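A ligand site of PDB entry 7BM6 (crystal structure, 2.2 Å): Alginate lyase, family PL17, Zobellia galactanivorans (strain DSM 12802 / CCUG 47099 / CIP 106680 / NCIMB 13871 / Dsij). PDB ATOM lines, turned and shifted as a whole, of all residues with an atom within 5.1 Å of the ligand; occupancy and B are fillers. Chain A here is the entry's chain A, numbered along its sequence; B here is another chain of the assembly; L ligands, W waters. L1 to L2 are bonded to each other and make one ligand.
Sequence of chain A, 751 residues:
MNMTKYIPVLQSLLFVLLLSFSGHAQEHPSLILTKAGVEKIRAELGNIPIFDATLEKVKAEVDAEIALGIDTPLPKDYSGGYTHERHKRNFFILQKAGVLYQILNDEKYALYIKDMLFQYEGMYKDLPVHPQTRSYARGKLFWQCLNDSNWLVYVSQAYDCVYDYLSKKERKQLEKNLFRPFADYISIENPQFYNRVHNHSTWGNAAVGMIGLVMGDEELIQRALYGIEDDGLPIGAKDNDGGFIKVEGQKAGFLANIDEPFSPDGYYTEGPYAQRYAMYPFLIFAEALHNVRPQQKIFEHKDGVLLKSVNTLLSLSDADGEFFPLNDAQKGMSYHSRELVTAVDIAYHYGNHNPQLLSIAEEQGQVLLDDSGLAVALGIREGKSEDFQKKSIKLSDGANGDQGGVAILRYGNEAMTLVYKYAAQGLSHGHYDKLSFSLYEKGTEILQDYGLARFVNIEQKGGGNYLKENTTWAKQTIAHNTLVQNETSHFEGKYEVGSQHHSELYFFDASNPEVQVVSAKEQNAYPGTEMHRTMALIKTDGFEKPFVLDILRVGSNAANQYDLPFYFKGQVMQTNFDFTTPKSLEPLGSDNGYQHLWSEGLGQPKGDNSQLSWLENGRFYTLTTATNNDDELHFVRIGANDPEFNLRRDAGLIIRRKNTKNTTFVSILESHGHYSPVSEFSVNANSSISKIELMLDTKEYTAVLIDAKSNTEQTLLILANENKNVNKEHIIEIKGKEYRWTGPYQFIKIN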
ATOM      1  N   LYS A  88     -20.284  -5.299 -14.479  1.00  0.00           N
ATOM      2  CA  LYS A  88     -20.243  -6.457 -13.577  1.00  0.00           C
ATOM      3  C   LYS A  88     -20.149  -5.953 -12.162  1.00  0.00           C
ATOM      4  O   LYS A  88     -20.883  -6.390 -11.249  1.00  0.00           O
ATOM      5  CB  LYS A  88     -19.071  -7.350 -13.952  1.00  0.00           C
ATOM      6  CG  LYS A  88     -18.873  -8.620 -13.149  1.00  0.00           C
ATOM      7  CD  LYS A  88     -17.606  -9.318 -13.652  1.00  0.00           C
ATOM      8  CE  LYS A  88     -17.465 -10.676 -12.990  1.00  0.00           C
ATOM      9  NZ  LYS A  88     -16.254 -11.462 -13.332  1.00  0.00           N
ATOM     10  N   TRP A 143     -20.788  -8.872 -23.727  1.00  0.00           N
ATOM     11  CA  TRP A 143     -20.543  -9.625 -24.949  1.00  0.00           C
ATOM     12  C   TRP A 143     -21.424 -10.867 -25.095  1.00  0.00           C
ATOM     13  O   TRP A 143     -21.683 -11.324 -26.216  1.00  0.00           O
ATOM     14  CB  TRP A 143     -19.031  -9.987 -25.032  1.00  0.00           C
ATOM     15  CG  TRP A 143     -18.579 -11.121 -24.154  1.00  0.00           C
ATOM     16  CD1 TRP A 143     -18.386 -11.101 -22.803  1.00  0.00           C
ATOM     17  CD2 TRP A 143     -18.312 -12.450 -24.583  1.00  0.00           C
ATOM     18  NE1 TRP A 143     -18.019 -12.351 -22.365  1.00  0.00           N
ATOM     19  CE2 TRP A 143     -17.918 -13.184 -23.451  1.00  0.00           C
ATOM     20  CE3 TRP A 143     -18.350 -13.090 -25.834  1.00  0.00           C
ATOM     21  CZ2 TRP A 143     -17.573 -14.534 -23.518  1.00  0.00           C
ATOM     22  CZ3 TRP A 143     -17.983 -14.422 -25.910  1.00  0.00           C
ATOM     23  CH2 TRP A 143     -17.589 -15.131 -24.756  1.00  0.00           C
ATOM     24  N   GLN A 144     -21.942 -11.381 -23.980  1.00  0.00           N
ATOM     25  CA  GLN A 144     -22.775 -12.550 -24.048  1.00  0.00           C
ATOM     26  C   GLN A 144     -23.962 -12.468 -23.052  1.00  0.00           C
ATOM     27  O   GLN A 144     -23.901 -11.837 -21.954  1.00  0.00           O
ATOM     28  CB  GLN A 144     -21.926 -13.830 -23.814  1.00  0.00           C
ATOM     29  CG  GLN A 144     -21.263 -13.800 -22.463  1.00  0.00           C
ATOM     30  CD  GLN A 144     -20.503 -15.080 -22.099  1.00  0.00           C
ATOM     31  OE1 GLN A 144     -20.559 -16.088 -22.764  1.00  0.00           O
ATOM     32  NE2 GLN A 144     -19.757 -14.978 -21.041  1.00  0.00           N
ATOM     33  N   LEU A 146     -25.060 -14.789 -21.145  1.00  0.00           N
ATOM     34  CA  LEU A 146     -24.666 -15.303 -19.824  1.00  0.00           C
ATOM     35  C   LEU A 146     -24.479 -14.166 -18.822  1.00  0.00           C
ATOM     36  O   LEU A 146     -24.981 -14.231 -17.679  1.00  0.00           O
ATOM     37  CB  LEU A 146     -23.415 -16.145 -19.898  1.00  0.00           C
ATOM     38  CG  LEU A 146     -22.858 -16.672 -18.578  1.00  0.00           C
ATOM     39  CD1 LEU A 146     -23.905 -17.457 -17.797  1.00  0.00           C
ATOM     40  CD2 LEU A 146     -21.561 -17.452 -18.803  1.00  0.00           C
ATOM     41  N   ASN A 147     -23.728 -13.147 -19.218  1.00  0.00           N
ATOM     42  CA  ASN A 147     -23.361 -12.075 -18.277  1.00  0.00           C
ATOM     43  C   ASN A 147     -24.529 -11.070 -18.080  1.00  0.00           C
ATOM     44  O   ASN A 147     -24.687 -10.570 -16.977  1.00  0.00           O
ATOM     45  CB  ASN A 147     -22.048 -11.363 -18.695  1.00  0.00           C
ATOM     46  CG  ASN A 147     -20.836 -12.273 -18.751  1.00  0.00           C
ATOM     47  OD1 ASN A 147     -20.113 -12.243 -19.719  1.00  0.00           O
ATOM     48  ND2 ASN A 147     -20.579 -13.023 -17.711  1.00  0.00           N
ATOM     49  N   ASN A 150     -26.408 -12.898 -15.394  1.00  0.00           N
ATOM     50  CA  ASN A 150     -25.743 -12.642 -14.075  1.00  0.00           C
ATOM     51  C   ASN A 150     -26.262 -11.325 -13.503  1.00  0.00           C
ATOM     52  O   ASN A 150     -26.673 -11.244 -12.342  1.00  0.00           O
ATOM     53  CB  ASN A 150     -24.213 -12.462 -14.149  1.00  0.00           C
ATOM     54  CG  ASN A 150     -23.423 -13.633 -14.693  1.00  0.00           C
ATOM     55  OD1 ASN A 150     -22.391 -13.389 -15.348  1.00  0.00           O
ATOM     56  ND2 ASN A 150     -23.848 -14.847 -14.479  1.00  0.00           N
ATOM     57  N   HIS A 198     -27.965 -26.769 -19.539  1.00  0.00           N
ATOM     58  CA  HIS A 198     -26.676 -26.141 -19.583  1.00  0.00           C
ATOM     59  C   HIS A 198     -26.600 -25.064 -18.515  1.00  0.00           C
ATOM     60  O   HIS A 198     -27.643 -24.446 -18.223  1.00  0.00           O
ATOM     61  CB  HIS A 198     -26.524 -25.494 -20.956  1.00  0.00           C
ATOM     62  CG  HIS A 198     -25.121 -25.162 -21.331  1.00  0.00           C
ATOM     63  ND1 HIS A 198     -24.544 -23.945 -21.040  1.00  0.00           N
ATOM     64  CD2 HIS A 198     -24.196 -25.830 -22.059  1.00  0.00           C
ATOM     65  CE1 HIS A 198     -23.317 -23.899 -21.504  1.00  0.00           C
ATOM     66  NE2 HIS A 198     -23.085 -25.024 -22.153  1.00  0.00           N
ATOM     67  N   ASN A 199     -25.429 -24.845 -17.920  1.00  0.00           N
ATOM     68  CA  ASN A 199     -25.233 -23.783 -16.945  1.00  0.00           C
ATOM     69  C   ASN A 199     -25.669 -22.374 -17.429  1.00  0.00           C
ATOM     70  O   ASN A 199     -26.209 -21.594 -16.653  1.00  0.00           O
ATOM     71  CB  ASN A 199     -23.825 -23.756 -16.312  1.00  0.00           C
ATOM     72  CG  ASN A 199     -22.765 -23.080 -17.177  1.00  0.00           C
ATOM     73  OD1 ASN A 199     -22.668 -21.851 -17.227  1.00  0.00           O
ATOM     74  ND2 ASN A 199     -21.955 -23.875 -17.834  1.00  0.00           N
ATOM     75  N   HIS A 200     -25.443 -22.078 -18.697  1.00  0.00           N
ATOM     76  CA  HIS A 200     -25.992 -20.862 -19.303  1.00  0.00           C
ATOM     77  C   HIS A 200     -27.475 -20.704 -19.069  1.00  0.00           C
ATOM     78  O   HIS A 200     -27.917 -19.632 -18.683  1.00  0.00           O
ATOM     79  CB  HIS A 200     -25.738 -20.786 -20.806  1.00  0.00           C
ATOM     80  CG  HIS A 200     -24.320 -20.519 -21.169  1.00  0.00           C
ATOM     81  ND1 HIS A 200     -23.936 -20.030 -22.412  1.00  0.00           N
ATOM     82  CD2 HIS A 200     -23.185 -20.650 -20.456  1.00  0.00           C
ATOM     83  CE1 HIS A 200     -22.629 -19.862 -22.423  1.00  0.00           C
ATOM     84  NE2 HIS A 200     -22.144 -20.287 -21.273  1.00  0.00           N
ATOM     85  N   ASP A 241     -18.294 -23.481 -28.038  1.00  0.00           N
ATOM     86  CA  ASP A 241     -17.431 -24.463 -27.412  1.00  0.00           C
ATOM     87  C   ASP A 241     -17.641 -25.904 -27.961  1.00  0.00           C
ATOM     88  O   ASP A 241     -17.128 -26.873 -27.379  1.00  0.00           O
ATOM     89  CB  ASP A 241     -17.636 -24.367 -25.903  1.00  0.00           C
ATOM     90  CG  ASP A 241     -17.498 -22.907 -25.367  1.00  0.00           C
ATOM     91  OD1 ASP A 241     -16.685 -22.103 -25.887  1.00  0.00           O
ATOM     92  OD2 ASP A 241     -18.225 -22.533 -24.452  1.00  0.00           O
ATOM     93  N   GLU A 270     -21.164 -31.467 -15.747  1.00  0.00           N
ATOM     94  CA  GLU A 270     -20.125 -30.648 -16.338  1.00  0.00           C
ATOM     95  C   GLU A 270     -18.839 -30.602 -15.487  1.00  0.00           C
ATOM     96  O   GLU A 270     -17.802 -30.221 -15.997  1.00  0.00           O
ATOM     97  CB  GLU A 270     -20.619 -29.224 -16.576  1.00  0.00           C
ATOM     98  CG  GLU A 270     -21.849 -29.051 -17.456  1.00  0.00           C
ATOM     99  CD  GLU A 270     -22.084 -27.556 -17.846  1.00  0.00           C
ATOM    100  OE1 GLU A 270     -21.205 -26.972 -18.501  1.00  0.00           O
ATOM    101  OE2 GLU A 270     -23.120 -26.954 -17.536  1.00  0.00           O
ATOM    102  N   TYR A 273     -15.800 -27.291 -11.498  1.00  0.00           N
ATOM    103  CA  TYR A 273     -15.577 -25.888 -11.787  1.00  0.00           C
ATOM    104  C   TYR A 273     -16.879 -25.253 -12.248  1.00  0.00           C
ATOM    105  O   TYR A 273     -17.289 -24.180 -11.741  1.00  0.00           O
ATOM    106  CB  TYR A 273     -14.450 -25.719 -12.802  1.00  0.00           C
ATOM    107  CG  TYR A 273     -14.241 -24.292 -13.242  1.00  0.00           C
ATOM    108  CD1 TYR A 273     -13.447 -23.391 -12.476  1.00  0.00           C
ATOM    109  CD2 TYR A 273     -14.819 -23.828 -14.448  1.00  0.00           C
ATOM    110  CE1 TYR A 273     -13.245 -22.073 -12.917  1.00  0.00           C
ATOM    111  CE2 TYR A 273     -14.626 -22.499 -14.865  1.00  0.00           C
ATOM    112  CZ  TYR A 273     -13.853 -21.630 -14.118  1.00  0.00           C
ATOM    113  OH  TYR A 273     -13.725 -20.309 -14.592  1.00  0.00           O
ATOM    114  N   ARG A 276     -19.684 -25.322  -9.370  1.00  0.00           N
ATOM    115  CA  ARG A 276     -19.467 -24.161  -8.551  1.00  0.00           C
ATOM    116  C   ARG A 276     -20.213 -22.905  -9.099  1.00  0.00           C
ATOM    117  O   ARG A 276     -20.806 -22.116  -8.358  1.00  0.00           O
ATOM    118  CB  ARG A 276     -17.945 -23.900  -8.449  1.00  0.00           C
ATOM    119  CG  ARG A 276     -17.510 -22.566  -7.830  1.00  0.00           C
ATOM    120  CD  ARG A 276     -17.495 -21.352  -8.760  1.00  0.00           C
ATOM    121  NE  ARG A 276     -16.977 -21.659 -10.080  1.00  0.00           N
ATOM    122  CZ  ARG A 276     -16.797 -20.770 -11.079  1.00  0.00           C
ATOM    123  NH1 ARG A 276     -17.075 -19.481 -10.938  1.00  0.00           N
ATOM    124  NH2 ARG A 276     -16.338 -21.171 -12.254  1.00  0.00           N
ATOM    125  N   TYR A 277     -20.124 -22.699 -10.399  1.00  0.00           N
ATOM    126  CA  TYR A 277     -20.692 -21.498 -11.005  1.00  0.00           C
ATOM    127  C   TYR A 277     -22.228 -21.624 -10.968  1.00  0.00           C
ATOM    128  O   TYR A 277     -22.933 -20.664 -10.639  1.00  0.00           O
ATOM    129  CB  TYR A 277     -20.194 -21.414 -12.444  1.00  0.00           C
ATOM    130  CG  TYR A 277     -20.508 -20.159 -13.187  1.00  0.00           C
ATOM    131  CD1 TYR A 277     -20.378 -18.908 -12.581  1.00  0.00           C
ATOM    132  CD2 TYR A 277     -21.000 -20.214 -14.497  1.00  0.00           C
ATOM    133  CE1 TYR A 277     -20.672 -17.737 -13.285  1.00  0.00           C
ATOM    134  CE2 TYR A 277     -21.308 -19.038 -15.192  1.00  0.00           C
ATOM    135  CZ  TYR A 277     -21.143 -17.811 -14.585  1.00  0.00           C
ATOM    136  OH  TYR A 277     -21.455 -16.664 -15.260  1.00  0.00           O
ATOM    137  N   HIS A 429     -17.986 -28.514 -22.389  1.00  0.00           N
ATOM    138  CA  HIS A 429     -16.700 -28.328 -21.773  1.00  0.00           C
ATOM    139  C   HIS A 429     -15.996 -29.615 -21.395  1.00  0.00           C
ATOM    140  O   HIS A 429     -14.916 -29.556 -20.813  1.00  0.00           O
ATOM    141  CB  HIS A 429     -16.844 -27.441 -20.523  1.00  0.00           C
ATOM    142  CG  HIS A 429     -17.374 -26.098 -20.838  1.00  0.00           C
ATOM    143  ND1 HIS A 429     -16.766 -25.270 -21.756  1.00  0.00           N
ATOM    144  CD2 HIS A 429     -18.479 -25.442 -20.415  1.00  0.00           C
ATOM    145  CE1 HIS A 429     -17.459 -24.145 -21.860  1.00  0.00           C
ATOM    146  NE2 HIS A 429     -18.500 -24.221 -21.062  1.00  0.00           N
ATOM    147  N   ARG A 454      -7.084 -21.000 -20.894  1.00  0.00           N
ATOM    148  CA  ARG A 454      -7.896 -19.790 -20.754  1.00  0.00           C
ATOM    149  C   ARG A 454      -7.439 -19.137 -19.484  1.00  0.00           C
ATOM    150  O   ARG A 454      -7.167 -19.830 -18.506  1.00  0.00           O
ATOM    151  CB  ARG A 454      -9.405 -20.136 -20.617  1.00  0.00           C
ATOM    152  CG  ARG A 454     -10.331 -18.941 -20.450  1.00  0.00           C
ATOM    153  CD  ARG A 454     -11.781 -19.342 -20.430  1.00  0.00           C
ATOM    154  NE  ARG A 454     -12.680 -18.237 -20.034  1.00  0.00           N
ATOM    155  CZ  ARG A 454     -13.800 -18.381 -19.321  1.00  0.00           C
ATOM    156  NH1 ARG A 454     -14.187 -19.568 -18.860  1.00  0.00           N
ATOM    157  NH2 ARG A 454     -14.485 -17.316 -19.000  1.00  0.00           N
ATOM    158  N   VAL A 456      -9.038 -16.791 -17.158  1.00  0.00           N
ATOM    159  CA  VAL A 456     -10.445 -16.350 -17.035  1.00  0.00           C
ATOM    160  C   VAL A 456     -10.532 -14.838 -16.702  1.00  0.00           C
ATOM    161  O   VAL A 456     -10.035 -14.373 -15.685  1.00  0.00           O
ATOM    162  CB  VAL A 456     -11.222 -17.247 -16.038  1.00  0.00           C
ATOM    163  CG1 VAL A 456     -12.632 -16.730 -15.785  1.00  0.00           C
ATOM    164  CG2 VAL A 456     -11.305 -18.677 -16.557  1.00  0.00           C
ATOM    165  N   ASN A 457     -11.145 -14.051 -17.599  1.00  0.00           N
ATOM    166  CA  ASN A 457     -11.342 -12.616 -17.409  1.00  0.00           C
ATOM    167  C   ASN A 457     -10.078 -11.761 -17.438  1.00  0.00           C
ATOM    168  O   ASN A 457     -10.107 -10.573 -16.994  1.00  0.00           O
ATOM    169  CB  ASN A 457     -12.144 -12.262 -16.122  1.00  0.00           C
ATOM    170  CG  ASN A 457     -13.477 -12.929 -16.027  1.00  0.00           C
ATOM    171  OD1 ASN A 457     -14.163 -13.205 -17.036  1.00  0.00           O
ATOM    172  ND2 ASN A 457     -13.893 -13.177 -14.786  1.00  0.00           N
ATOM    173  N   TYR A 466     -11.967 -18.558 -23.984  1.00  0.00           N
ATOM    174  CA  TYR A 466     -11.291 -19.803 -24.391  1.00  0.00           C
ATOM    175  C   TYR A 466     -10.322 -19.505 -25.525  1.00  0.00           C
ATOM    176  O   TYR A 466     -10.652 -18.747 -26.483  1.00  0.00           O
ATOM    177  CB  TYR A 466     -12.322 -20.909 -24.773  1.00  0.00           C
ATOM    178  CG  TYR A 466     -12.871 -21.500 -23.509  1.00  0.00           C
ATOM    179  CD1 TYR A 466     -12.077 -22.288 -22.702  1.00  0.00           C
ATOM    180  CD2 TYR A 466     -14.149 -21.171 -23.044  1.00  0.00           C
ATOM    181  CE1 TYR A 466     -12.539 -22.803 -21.471  1.00  0.00           C
ATOM    182  CE2 TYR A 466     -14.608 -21.645 -21.806  1.00  0.00           C
ATOM    183  CZ  TYR A 466     -13.797 -22.471 -21.033  1.00  0.00           C
ATOM    184  OH  TYR A 466     -14.197 -22.921 -19.790  1.00  0.00           O
ATOM    185  N   GLU B 680     -11.964 -14.400  -9.735  1.00  0.00           N
ATOM    186  CA  GLU B 680     -11.804 -14.209 -11.198  1.00  0.00           C
ATOM    187  C   GLU B 680     -11.779 -12.727 -11.682  1.00  0.00           C
ATOM    188  O   GLU B 680     -12.066 -12.464 -12.848  1.00  0.00           O
ATOM    189  CB  GLU B 680     -12.786 -15.072 -11.960  1.00  0.00           C
ATOM    190  CG  GLU B 680     -12.624 -16.551 -11.642  1.00  0.00           C
ATOM    191  CD  GLU B 680     -13.430 -17.485 -12.514  1.00  0.00           C
ATOM    192  OE1 GLU B 680     -14.559 -17.098 -12.976  1.00  0.00           O
ATOM    193  OE2 GLU B 680     -12.889 -18.595 -12.773  1.00  0.00           O
HETATM  194  C1  LIG L   1     -18.755 -20.056 -22.570  1.00  0.00           C
HETATM  195  O1  LIG L   1     -17.521 -20.611 -23.004  1.00  0.00           O
HETATM  196  C2  LIG L   1     -18.524 -18.624 -22.107  1.00  0.00           C
HETATM  197  O2  LIG L   1     -19.806 -18.142 -21.750  1.00  0.00           O
HETATM  198  C3  LIG L   1     -17.670 -18.581 -20.850  1.00  0.00           C
HETATM  199  O3  LIG L   1     -17.630 -17.240 -20.325  1.00  0.00           O
HETATM  200  C4  LIG L   1     -18.248 -19.499 -19.769  1.00  0.00           C
HETATM  201  O4  LIG L   1     -17.370 -19.577 -18.655  1.00  0.00           O
HETATM  202  C5  LIG L   1     -18.543 -20.900 -20.306  1.00  0.00           C
HETATM  203  O5  LIG L   1     -19.298 -20.847 -21.517  1.00  0.00           O
HETATM  204  C6  LIG L   1     -19.366 -21.624 -19.244  1.00  0.00           C
HETATM  205  O6  LIG L   1     -18.987 -21.665 -18.062  1.00  0.00           O
HETATM  206  O7  LIG L   1     -20.428 -22.186 -19.563  1.00  0.00           O
HETATM  207  C1  LG2 L   2     -17.733 -19.093 -17.329  1.00  0.00           C
HETATM  208  C2  LG2 L   2     -16.997 -19.497 -16.052  1.00  0.00           C
HETATM  209  O1  LG2 L   2     -15.603 -19.271 -16.271  1.00  0.00           O
HETATM  210  C3  LG2 L   2     -17.430 -18.706 -14.826  1.00  0.00           C
HETATM  211  O2  LG2 L   2     -16.479 -18.867 -13.767  1.00  0.00           O
HETATM  212  C4  LG2 L   2     -17.599 -17.225 -15.156  1.00  0.00           C
HETATM  213  C5  LG2 L   2     -17.715 -16.779 -16.421  1.00  0.00           C
HETATM  214  O3  LG2 L   2     -17.609 -17.668 -17.561  1.00  0.00           O
HETATM  215  C6  LG2 L   2     -17.970 -15.348 -16.730  1.00  0.00           C
HETATM  216  O4  LG2 L   2     -18.038 -14.475 -15.843  1.00  0.00           O
HETATM  217  O5  LG2 L   2     -18.130 -15.025 -17.912  1.00  0.00           O
HETATM  218  O   HOH W   1     -19.961 -14.482 -14.242  1.00  0.00           O
HETATM  219  O   HOH W   2     -17.026 -13.387 -19.878  1.00  0.00           O
HETATM  220  O   HOH W   3     -16.835 -12.191 -16.458  1.00  0.00           O
HETATM  221  O   HOH W   4     -15.290 -16.685 -21.895  1.00  0.00           O
HETATM  222  O   HOH W   5     -17.371 -18.871 -25.817  1.00  0.00           O
HETATM  223  O   HOH W   6     -16.100 -14.650 -13.879  1.00  0.00           O
HETATM  224  O   HOH W   7     -16.152 -22.296 -18.460  1.00  0.00           O
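The side-chain amide oxygen (OE1) of Gln 144 lies within hydrogen-bond range of an oxygen (O2) of LIG L1 (2.4 Å). O1 of LIG L1 lies within hydrogen-bond range of OD2 of Asp 241, at 2.5 Å. An oxygen (O1) of LG2 L2 lies within hydrogen-bond range of the side-chain hydroxyl of Tyr 273, 2.7 Å away. OE1 of Glu 680 of chain B is in hydrogen-bond range of O2 of LG2 L2 (2.7 Å). NH2 of Arg 276 sits at hydrogen-bond distance from O2 of LG2 L2 (2.8 Å). An oxygen (O7) of LIG L1 sits at hydrogen-bond distance from the side-chain amide nitrogen (ND2) of Asn 199 (2.9 Å). An oxygen (O5) of LIG L1 lies within hydrogen-bond range of a ring nitrogen (NE2) of His 200 (2.9 Å). NH1 of Arg 454 lies within hydrogen-bond range of O1 of LG2 L2, at 3.0 Å. The side-chain amide nitrogen (ND2) of Asn 147 is in hydrogen-bond range of an oxygen (O5) of LG2 L2. An oxygen (O7) of LIG L1 lies within hydrogen-bond range of a ring nitrogen (NE2) of His 429 (3.2 Å).
The side-chain amide nitrogen (NE2) of Gln 144 is in hydrogen-bond range of the side-chain amide oxygen (OD1) of Asn 147 (3.1 Å). NE2 of Gln 144 sits close to NE1 of Trp 143 (3.4 Å). The side-chain hydroxyl (OH) of Tyr 273 is in hydrogen-bond range of the side-chain carboxylate (OE2) of Glu 680 of chain B, at 2.6 Å. The backbone NH of Asn 199 sits at hydrogen-bond distance from the side-chain carboxylate of Glu 270 (3.2 Å). A ring nitrogen (ND1) of His 198 lies within hydrogen-bond range of the backbone NH of His 200 (3.1 Å). OH of Tyr 466 sits at hydrogen-bond distance from NH1 of Arg 454. The side-chain amide oxygen of Asn 150 sits at hydrogen-bond distance from the side-chain amide nitrogen of Asn 147, at 3.0 Å. ND2 of Asn 150 sits at hydrogen-bond distance from OH of Tyr 277, at 3.1 Å.
Residues that only touch the ligand: Leu 146, His 198, Tyr 277, Val 456 and Tyr 466. Hydrophobic or aromatic side chains within 4 Å of the ligand: Leu 146, His 198, His 200, Tyr 273, Tyr 277, His 429, Val 456 and Tyr 466. The nearest printed residue that does not touch the ligand is Trp 143 (4.2 Å).
Water W1 lies within hydrogen-bond range of an oxygen (O4) of LG2 L2 (2.5 Å), the side-chain hydroxyl (OH) of Tyr 277 (2.8 Å) and the side-chain amide oxygen (OD1) of Asn 150 (2.9 Å). Water W3 lies within hydrogen-bond range of an oxygen (O4) of LG2 L2 (2.7 Å), the side-chain amide oxygen (OD1) of Asn 457 (2.9 Å) and the side-chain amino group (NZ) of Lys 88 (3.3 Å). Water W6 lies within hydrogen-bond range of an oxygen (O4) of LG2 L2 (2.8 Å), the side-chain amide nitrogen (ND2) of Asn 457 (2.8 Å), the side-chain carboxylate (OE1) of Glu 680 of chain B (3.0 Å) and the side-chain amino group (NZ) of Lys 88 (3.2 Å). Water W4 lies within hydrogen-bond range of O3 of LIG L1 and NH2 of Arg 454. Water W7 lies within hydrogen-bond range of the side-chain hydroxyl of Tyr 466, an oxygen (O6) of LIG L1 and the guanidinium group of Arg 454. Water W5 bridges OD1 of Asp 241 and O1 of LIG L1.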
